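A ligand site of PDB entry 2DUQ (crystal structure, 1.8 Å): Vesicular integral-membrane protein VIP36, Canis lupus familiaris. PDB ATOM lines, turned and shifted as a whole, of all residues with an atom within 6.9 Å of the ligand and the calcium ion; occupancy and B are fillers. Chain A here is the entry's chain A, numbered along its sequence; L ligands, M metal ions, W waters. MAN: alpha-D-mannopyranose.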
ATOM      1  N   SER A  48     -16.959 -23.038 -11.357  1.00  0.00           N
ATOM      2  CA  SER A  48     -17.585 -22.119 -10.404  1.00  0.00           C
ATOM      3  C   SER A  48     -17.765 -20.730 -10.999  1.00  0.00           C
ATOM      4  O   SER A  48     -17.382 -19.732 -10.368  1.00  0.00           O
ATOM      5  CB  SER A  48     -16.796 -22.049  -9.105  1.00  0.00           C
ATOM      6  OG  SER A  48     -16.683 -23.345  -8.531  1.00  0.00           O
ATOM      7  N   HIS A  81     -18.810 -32.655 -17.615  1.00  0.00           N
ATOM      8  CA  HIS A  81     -19.078 -31.303 -18.112  1.00  0.00           C
ATOM      9  C   HIS A  81     -20.365 -30.774 -17.472  1.00  0.00           C
ATOM     10  O   HIS A  81     -21.193 -31.552 -16.983  1.00  0.00           O
ATOM     11  CB  HIS A  81     -19.171 -31.275 -19.631  1.00  0.00           C
ATOM     12  CG  HIS A  81     -20.158 -32.250 -20.187  1.00  0.00           C
ATOM     13  ND1 HIS A  81     -19.801 -33.508 -20.606  1.00  0.00           N
ATOM     14  CD2 HIS A  81     -21.497 -32.168 -20.356  1.00  0.00           C
ATOM     15  CE1 HIS A  81     -20.863 -34.154 -21.028  1.00  0.00           C
ATOM     16  NE2 HIS A  81     -21.916 -33.363 -20.886  1.00  0.00           N
ATOM     17  N   GLY A  82     -20.514 -29.455 -17.429  1.00  0.00           N
ATOM     18  CA  GLY A  82     -21.717 -28.835 -16.877  1.00  0.00           C
ATOM     19  C   GLY A  82     -21.600 -27.309 -16.912  1.00  0.00           C
ATOM     20  O   GLY A  82     -20.543 -26.797 -17.239  1.00  0.00           O
ATOM     21  N   ASP A  83     -22.648 -26.586 -16.562  1.00  0.00           N
ATOM     22  CA  ASP A  83     -23.932 -27.163 -16.124  1.00  0.00           C
ATOM     23  C   ASP A  83     -25.036 -26.931 -17.135  1.00  0.00           C
ATOM     24  O   ASP A  83     -26.066 -27.642 -17.093  1.00  0.00           O
ATOM     25  CB  ASP A  83     -24.315 -26.575 -14.772  1.00  0.00           C
ATOM     26  CG  ASP A  83     -23.704 -27.329 -13.635  1.00  0.00           C
ATOM     27  OD1 ASP A  83     -22.648 -26.874 -13.144  1.00  0.00           O
ATOM     28  OD2 ASP A  83     -24.228 -28.403 -13.293  1.00  0.00           O
ATOM     29  N   PRO A  98     -28.209 -19.514  -8.594  1.00  0.00           N
ATOM     30  CA  PRO A  98     -27.951 -20.943  -8.765  1.00  0.00           C
ATOM     31  C   PRO A  98     -28.650 -21.561  -9.971  1.00  0.00           C
ATOM     32  O   PRO A  98     -28.391 -22.723 -10.289  1.00  0.00           O
ATOM     33  CB  PRO A  98     -28.498 -21.521  -7.454  1.00  0.00           C
ATOM     34  CG  PRO A  98     -29.658 -20.648  -7.127  1.00  0.00           C
ATOM     35  CD  PRO A  98     -29.267 -19.263  -7.596  1.00  0.00           C
ATOM     36  N   PHE A 100     -28.671 -21.926 -13.470  1.00  0.00           N
ATOM     37  CA  PHE A 100     -27.774 -21.750 -14.620  1.00  0.00           C
ATOM     38  C   PHE A 100     -27.195 -20.366 -14.667  1.00  0.00           C
ATOM     39  O   PHE A 100     -27.249 -19.691 -15.694  1.00  0.00           O
ATOM     40  CB  PHE A 100     -28.478 -22.154 -15.931  1.00  0.00           C
ATOM     41  CG  PHE A 100     -29.005 -23.558 -15.900  1.00  0.00           C
ATOM     42  CD1 PHE A 100     -28.182 -24.629 -16.173  1.00  0.00           C
ATOM     43  CD2 PHE A 100     -30.333 -23.798 -15.552  1.00  0.00           C
ATOM     44  CE1 PHE A 100     -28.666 -25.941 -16.109  1.00  0.00           C
ATOM     45  CE2 PHE A 100     -30.819 -25.093 -15.502  1.00  0.00           C
ATOM     46  CZ  PHE A 100     -29.985 -26.171 -15.763  1.00  0.00           C
ATOM     47  N   ASP A 114     -30.004 -28.119 -19.990  1.00  0.00           N
ATOM     48  CA  ASP A 114     -29.273 -28.727 -18.880  1.00  0.00           C
ATOM     49  C   ASP A 114     -28.355 -29.840 -19.387  1.00  0.00           C
ATOM     50  O   ASP A 114     -28.831 -30.797 -19.988  1.00  0.00           O
ATOM     51  CB  ASP A 114     -30.320 -29.297 -17.897  1.00  0.00           C
ATOM     52  CG  ASP A 114     -29.704 -29.740 -16.588  1.00  0.00           C
ATOM     53  OD1 ASP A 114     -30.493 -29.992 -15.645  1.00  0.00           O
ATOM     54  OD2 ASP A 114     -28.455 -29.815 -16.454  1.00  0.00           O
ATOM     55  N   THR A 115     -27.060 -29.740 -19.115  1.00  0.00           N
ATOM     56  CA  THR A 115     -26.102 -30.708 -19.682  1.00  0.00           C
ATOM     57  C   THR A 115     -25.533 -31.696 -18.671  1.00  0.00           C
ATOM     58  O   THR A 115     -24.744 -32.566 -19.047  1.00  0.00           O
ATOM     59  CB  THR A 115     -24.897 -30.004 -20.321  1.00  0.00           C
ATOM     60  OG1 THR A 115     -24.173 -29.309 -19.294  1.00  0.00           O
ATOM     61  CG2 THR A 115     -25.344 -29.031 -21.449  1.00  0.00           C
ATOM     62  N   TYR A 116     -25.903 -31.553 -17.401  1.00  0.00           N
ATOM     63  CA  TYR A 116     -25.392 -32.448 -16.360  1.00  0.00           C
ATOM     64  C   TYR A 116     -26.537 -33.034 -15.519  1.00  0.00           C
ATOM     65  O   TYR A 116     -27.298 -32.285 -14.943  1.00  0.00           O
ATOM     66  CB  TYR A 116     -24.390 -31.697 -15.460  1.00  0.00           C
ATOM     67  CG  TYR A 116     -23.851 -32.571 -14.382  1.00  0.00           C
ATOM     68  CD1 TYR A 116     -23.121 -33.718 -14.692  1.00  0.00           C
ATOM     69  CD2 TYR A 116     -24.101 -32.282 -13.037  1.00  0.00           C
ATOM     70  CE1 TYR A 116     -22.643 -34.564 -13.702  1.00  0.00           C
ATOM     71  CE2 TYR A 116     -23.623 -33.133 -12.026  1.00  0.00           C
ATOM     72  CZ  TYR A 116     -22.895 -34.257 -12.372  1.00  0.00           C
ATOM     73  OH  TYR A 116     -22.418 -35.091 -11.374  1.00  0.00           O
ATOM     74  N   PRO A 117     -26.646 -34.393 -15.468  1.00  0.00           N
ATOM     75  CA  PRO A 117     -27.680 -34.988 -14.612  1.00  0.00           C
ATOM     76  C   PRO A 117     -27.301 -34.953 -13.141  1.00  0.00           C
ATOM     77  O   PRO A 117     -26.595 -35.856 -12.655  1.00  0.00           O
ATOM     78  CB  PRO A 117     -27.758 -36.456 -15.100  1.00  0.00           C
ATOM     79  CG  PRO A 117     -26.379 -36.755 -15.652  1.00  0.00           C
ATOM     80  CD  PRO A 117     -25.863 -35.418 -16.200  1.00  0.00           C
ATOM     81  N   ASN A 118     -27.762 -33.939 -12.430  1.00  0.00           N
ATOM     82  CA  ASN A 118     -27.566 -33.871 -10.979  1.00  0.00           C
ATOM     83  C   ASN A 118     -28.352 -34.954 -10.243  1.00  0.00           C
ATOM     84  O   ASN A 118     -27.977 -35.367  -9.150  1.00  0.00           O
ATOM     85  CB  ASN A 118     -27.972 -32.502 -10.452  1.00  0.00           C
ATOM     86  CG  ASN A 118     -27.058 -31.399 -10.934  1.00  0.00           C
ATOM     87  OD1 ASN A 118     -27.273 -30.850 -12.020  1.00  0.00           O
ATOM     88  ND2 ASN A 118     -26.056 -31.058 -10.134  1.00  0.00           N
ATOM     89  N   ASP A 119     -29.439 -35.387 -10.862  1.00  0.00           N
ATOM     90  CA  ASP A 119     -30.368 -36.290 -10.197  1.00  0.00           C
ATOM     91  C   ASP A 119     -29.822 -37.690 -10.378  1.00  0.00           C
ATOM     92  O   ASP A 119     -29.807 -38.205 -11.488  1.00  0.00           O
ATOM     93  CB  ASP A 119     -31.747 -36.176 -10.842  1.00  0.00           C
ATOM     94  CG  ASP A 119     -32.816 -36.967 -10.080  1.00  0.00           C
ATOM     95  OD1 ASP A 119     -32.468 -37.800  -9.229  1.00  0.00           O
ATOM     96  OD2 ASP A 119     -34.013 -36.753 -10.354  1.00  0.00           O
ATOM     97  N   PHE A 126     -29.520 -37.065 -21.098  1.00  0.00           N
ATOM     98  CA  PHE A 126     -28.980 -35.692 -21.184  1.00  0.00           C
ATOM     99  C   PHE A 126     -28.129 -35.437 -22.432  1.00  0.00           C
ATOM    100  O   PHE A 126     -27.604 -36.383 -23.034  1.00  0.00           O
ATOM    101  CB  PHE A 126     -28.191 -35.359 -19.897  1.00  0.00           C
ATOM    102  CG  PHE A 126     -29.080 -34.962 -18.752  1.00  0.00           C
ATOM    103  CD1 PHE A 126     -29.855 -35.925 -18.082  1.00  0.00           C
ATOM    104  CD2 PHE A 126     -29.172 -33.627 -18.354  1.00  0.00           C
ATOM    105  CE1 PHE A 126     -30.700 -35.569 -17.050  1.00  0.00           C
ATOM    106  CE2 PHE A 126     -30.019 -33.248 -17.306  1.00  0.00           C
ATOM    107  CZ  PHE A 126     -30.794 -34.205 -16.657  1.00  0.00           C
ATOM    108  N   TYR A 140     -36.169 -23.620  -8.251  1.00  0.00           N
ATOM    109  CA  TYR A 140     -35.665 -24.647  -9.143  1.00  0.00           C
ATOM    110  C   TYR A 140     -34.769 -25.579  -8.320  1.00  0.00           C
ATOM    111  O   TYR A 140     -33.781 -25.159  -7.731  1.00  0.00           O
ATOM    112  CB  TYR A 140     -34.866 -23.980 -10.263  1.00  0.00           C
ATOM    113  CG  TYR A 140     -34.135 -24.961 -11.159  1.00  0.00           C
ATOM    114  CD1 TYR A 140     -34.800 -25.638 -12.168  1.00  0.00           C
ATOM    115  CD2 TYR A 140     -32.747 -25.166 -11.005  1.00  0.00           C
ATOM    116  CE1 TYR A 140     -34.127 -26.533 -13.022  1.00  0.00           C
ATOM    117  CE2 TYR A 140     -32.075 -26.037 -11.844  1.00  0.00           C
ATOM    118  CZ  TYR A 140     -32.760 -26.713 -12.843  1.00  0.00           C
ATOM    119  OH  TYR A 140     -32.098 -27.600 -13.658  1.00  0.00           O
ATOM    120  N   HIS A 142     -32.055 -27.546  -8.298  1.00  0.00           N
ATOM    121  CA  HIS A 142     -30.895 -27.837  -9.132  1.00  0.00           C
ATOM    122  C   HIS A 142     -30.368 -29.270  -8.919  1.00  0.00           C
ATOM    123  O   HIS A 142     -30.030 -29.956  -9.884  1.00  0.00           O
ATOM    124  CB  HIS A 142     -29.822 -26.777  -8.887  1.00  0.00           C
ATOM    125  CG  HIS A 142     -28.532 -27.082  -9.583  1.00  0.00           C
ATOM    126  ND1 HIS A 142     -28.370 -26.981 -10.938  1.00  0.00           N
ATOM    127  CD2 HIS A 142     -27.348 -27.530  -9.098  1.00  0.00           C
ATOM    128  CE1 HIS A 142     -27.138 -27.338 -11.267  1.00  0.00           C
ATOM    129  NE2 HIS A 142     -26.508 -27.678 -10.163  1.00  0.00           N
ATOM    130  N   SER A 143     -30.363 -29.715  -7.654  1.00  0.00           N
ATOM    131  CA  SER A 143     -29.853 -31.063  -7.326  1.00  0.00           C
ATOM    132  C   SER A 143     -30.639 -32.178  -7.982  1.00  0.00           C
ATOM    133  O   SER A 143     -30.142 -33.314  -8.106  1.00  0.00           O
ATOM    134  CB  SER A 143     -29.807 -31.270  -5.812  1.00  0.00           C
ATOM    135  OG  SER A 143     -31.110 -31.470  -5.279  1.00  0.00           O
ATOM    136  N   LYS A 144     -31.873 -31.863  -8.400  1.00  0.00           N
ATOM    137  CA  LYS A 144     -32.772 -32.797  -9.035  1.00  0.00           C
ATOM    138  C   LYS A 144     -33.125 -32.383 -10.475  1.00  0.00           C
ATOM    139  O   LYS A 144     -34.131 -32.825 -11.018  1.00  0.00           O
ATOM    140  CB  LYS A 144     -34.028 -32.972  -8.148  1.00  0.00           C
ATOM    141  CG  LYS A 144     -33.770 -33.714  -6.826  1.00  0.00           C
ATOM    142  CD  LYS A 144     -33.350 -35.162  -7.144  1.00  0.00           C
ATOM    143  CE  LYS A 144     -33.942 -36.180  -6.213  1.00  0.00           C
ATOM    144  NZ  LYS A 144     -33.926 -37.543  -6.872  1.00  0.00           N
ATOM    145  N   ASP A 145     -32.291 -31.540 -11.099  1.00  0.00           N
ATOM    146  CA  ASP A 145     -32.497 -31.083 -12.484  1.00  0.00           C
ATOM    147  C   ASP A 145     -33.912 -30.519 -12.721  1.00  0.00           C
ATOM    148  O   ASP A 145     -34.472 -30.710 -13.797  1.00  0.00           O
ATOM    149  CB  ASP A 145     -32.227 -32.197 -13.515  1.00  0.00           C
ATOM    150  CG  ASP A 145     -30.893 -32.891 -13.283  1.00  0.00           C
ATOM    151  OD1 ASP A 145     -30.870 -34.150 -13.189  1.00  0.00           O
ATOM    152  OD2 ASP A 145     -29.885 -32.170 -13.174  1.00  0.00           O
ATOM    153  N   GLY A 146     -34.476 -29.898 -11.697  1.00  0.00           N
ATOM    154  CA  GLY A 146     -35.761 -29.189 -11.819  1.00  0.00           C
ATOM    155  C   GLY A 146     -36.955 -30.112 -11.951  1.00  0.00           C
ATOM    156  O   GLY A 146     -38.024 -29.719 -12.443  1.00  0.00           O
ATOM    157  N   GLY A 210     -24.004 -21.491 -16.093  1.00  0.00           N
ATOM    158  CA  GLY A 210     -23.325 -21.687 -14.854  1.00  0.00           C
ATOM    159  C   GLY A 210     -22.432 -22.894 -14.965  1.00  0.00           C
ATOM    160  O   GLY A 210     -22.729 -23.821 -15.731  1.00  0.00           O
ATOM    161  N   THR A 211     -21.308 -22.829 -14.260  1.00  0.00           N
ATOM    162  CA  THR A 211     -20.459 -24.008 -14.123  1.00  0.00           C
ATOM    163  C   THR A 211     -20.223 -24.218 -12.594  1.00  0.00           C
ATOM    164  O   THR A 211     -20.328 -23.270 -11.831  1.00  0.00           O
ATOM    165  CB  THR A 211     -19.085 -23.819 -14.836  1.00  0.00           C
ATOM    166  OG1 THR A 211     -18.379 -22.715 -14.251  1.00  0.00           O
ATOM    167  CG2 THR A 211     -19.230 -23.632 -16.358  1.00  0.00           C
ATOM    168  N   GLY A 212     -19.942 -25.456 -12.192  1.00  0.00           N
ATOM    169  CA  GLY A 212     -19.663 -25.822 -10.793  1.00  0.00           C
ATOM    170  C   GLY A 212     -18.325 -26.556 -10.757  1.00  0.00           C
ATOM    171  O   GLY A 212     -17.310 -26.005 -11.175  1.00  0.00           O
ATOM    172  N   ASP A 213     -18.336 -27.797 -10.268  1.00  0.00           N
ATOM    173  CA  ASP A 213     -17.120 -28.633 -10.286  1.00  0.00           C
ATOM    174  C   ASP A 213     -16.850 -29.042 -11.717  1.00  0.00           C
ATOM    175  O   ASP A 213     -15.718 -29.398 -12.059  1.00  0.00           O
ATOM    176  CB  ASP A 213     -17.272 -29.900  -9.427  1.00  0.00           C
ATOM    177  CG  ASP A 213     -17.412 -29.625  -7.945  1.00  0.00           C
ATOM    178  OD1 ASP A 213     -16.731 -28.710  -7.423  1.00  0.00           O
ATOM    179  OD2 ASP A 213     -18.204 -30.357  -7.291  1.00  0.00           O
ATOM    180  N   LEU A 214     -17.893 -28.973 -12.550  1.00  0.00           N
ATOM    181  CA  LEU A 214     -17.826 -29.343 -13.974  1.00  0.00           C
ATOM    182  C   LEU A 214     -18.075 -28.086 -14.788  1.00  0.00           C
ATOM    183  O   LEU A 214     -18.749 -27.160 -14.328  1.00  0.00           O
ATOM    184  CB  LEU A 214     -18.826 -30.431 -14.324  1.00  0.00           C
ATOM    185  CG  LEU A 214     -18.605 -31.721 -13.514  1.00  0.00           C
ATOM    186  CD1 LEU A 214     -19.755 -32.684 -13.750  1.00  0.00           C
ATOM    187  CD2 LEU A 214     -17.219 -32.392 -13.734  1.00  0.00           C
ATOM    188  N   SER A 215     -17.479 -28.043 -15.979  1.00  0.00           N
ATOM    189  CA  SER A 215     -17.537 -26.807 -16.764  1.00  0.00           C
ATOM    190  C   SER A 215     -17.738 -27.070 -18.266  1.00  0.00           C
ATOM    191  O   SER A 215     -17.790 -28.219 -18.706  1.00  0.00           O
ATOM    192  CB  SER A 215     -16.299 -25.936 -16.507  1.00  0.00           C
ATOM    193  OG  SER A 215     -15.114 -26.601 -16.927  1.00  0.00           O
HETATM  194  C1  MAN L   1     -20.831 -29.080  -8.058  1.00  0.00           C
HETATM  195  C2  MAN L   1     -22.004 -28.166  -7.730  1.00  0.00           C
HETATM  196  C3  MAN L   1     -23.242 -28.587  -8.538  1.00  0.00           C
HETATM  197  C4  MAN L   1     -22.916 -28.658 -10.038  1.00  0.00           C
HETATM  198  C5  MAN L   1     -21.740 -29.616 -10.235  1.00  0.00           C
HETATM  199  C6  MAN L   1     -21.319 -29.768 -11.716  1.00  0.00           C
HETATM  200  O1  MAN L   1     -21.029 -30.379  -7.490  1.00  0.00           O
HETATM  201  O2  MAN L   1     -21.643 -26.805  -7.960  1.00  0.00           O
HETATM  202  O3  MAN L   1     -24.312 -27.704  -8.293  1.00  0.00           O
HETATM  203  O4  MAN L   1     -24.033 -29.086 -10.770  1.00  0.00           O
HETATM  204  O5  MAN L   1     -20.636 -29.152  -9.469  1.00  0.00           O
HETATM  205  O6  MAN L   1     -20.712 -28.579 -12.171  1.00  0.00           O
HETATM  206 CA    CA M   1     -28.481 -30.482 -14.072  1.00  0.00          CA
HETATM  207  O   HOH W   1     -29.713 -28.716 -12.816  1.00  0.00           O
HETATM  208  O   HOH W   2     -24.023 -25.033  -9.293  1.00  0.00           O
HETATM  209  O   HOH W   3     -22.773 -32.394  -7.656  1.00  0.00           O
HETATM  210  O   HOH W   4     -19.865 -26.208  -6.043  1.00  0.00           O
HETATM  211  O   HOH W   5     -26.623 -28.993 -14.511  1.00  0.00           O
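ND2 of Asn 118 sits at hydrogen-bond distance from O4 of the ligand.
O4 of the ligand sits at hydrogen-bond distance from OD2 of Asp 83.
The backbone NH of Gly 212 lies within hydrogen-bond range of an oxygen (O6) of the ligand (3.2 Å).
O of Leu 214 sits at hydrogen-bond distance from O6 of the ligand (3.2 Å).
The backbone NH of Asp 213 is in hydrogen-bond range of an oxygen (O5) of the ligand, at 2.8 Å.
O6 of the ligand is in hydrogen-bond range of N of Leu 214, 2.9 Å away.
NE2 of His 142 sits at hydrogen-bond distance from O3 of the ligand.
An oxygen (O1) of the ligand is in hydrogen-bond range of the side-chain carboxylate (OD2) of Asp 213 (2.8 Å).
Water W1 bridges the side-chain hydroxyl (OH) of Tyr 140 (2.8 Å) and a ring nitrogen (ND1) of His 142 (2.9 Å).
The backbone carbonyl oxygen (O) of Tyr 116 binds the calcium ion, 2.3 Å away.
The calcium ion is bound by the side-chain carboxylate (OD2) of Asp 145, at 2.4 Å.
The calcium ion is bound by the side-chain amide oxygen (OD1) of Asn 118 (2.4 Å).
The calcium ion is bound by water W5.
The side-chain carboxylate (OD2) of Asp 114 is bound to the calcium ion, 2.5 Å away.
Water W1 is bound to the calcium ion, at 2.5 Å.
The calcium ion is bound by the side-chain carboxylate (OD1) of Asp 114.
The calcium ion has seven donor atoms within binding distance.
The nearest printed residue that does not touch the calcium ion is His 142 (4.4 Å).
The side-chain carboxylate (OD1) of Asp 114 lies close to the side-chain hydroxyl (OH) of Tyr 140 (3.5 Å).
The side-chain amide nitrogen (ND2) of Asn 118 is in hydrogen-bond range of a ring nitrogen (NE2) of His 142 (3.4 Å).
OD1 of Asp 145 sits at hydrogen-bond distance from N of Asp 119 (3.0 Å).
The backbone carbonyl oxygen of Asp 83 is in hydrogen-bond range of the backbone NH of Thr 115 (3.1 Å).
The backbone NH (N) of Ser 48 lies within hydrogen-bond range of the backbone carbonyl oxygen (O) of Gly 212 (3.0 Å).
The backbone NH (N) of Asp 83 sits at hydrogen-bond distance from the backbone carbonyl oxygen (O) of Gly 210 (2.9 Å).
The side-chain carboxylate (OD1) of Asp 83 lies within hydrogen-bond range of the backbone NH (N) of Gly 212, at 3.2 Å.
Hydrophobic or aromatic side chains that line the ligand: Tyr 116, His 142 and Leu 214.
Seven residues have an atom within 4 Å of the ligand: Asp 83, Tyr 116, Asn 118, His 142, Gly 212, Asp 213 and Leu 214.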
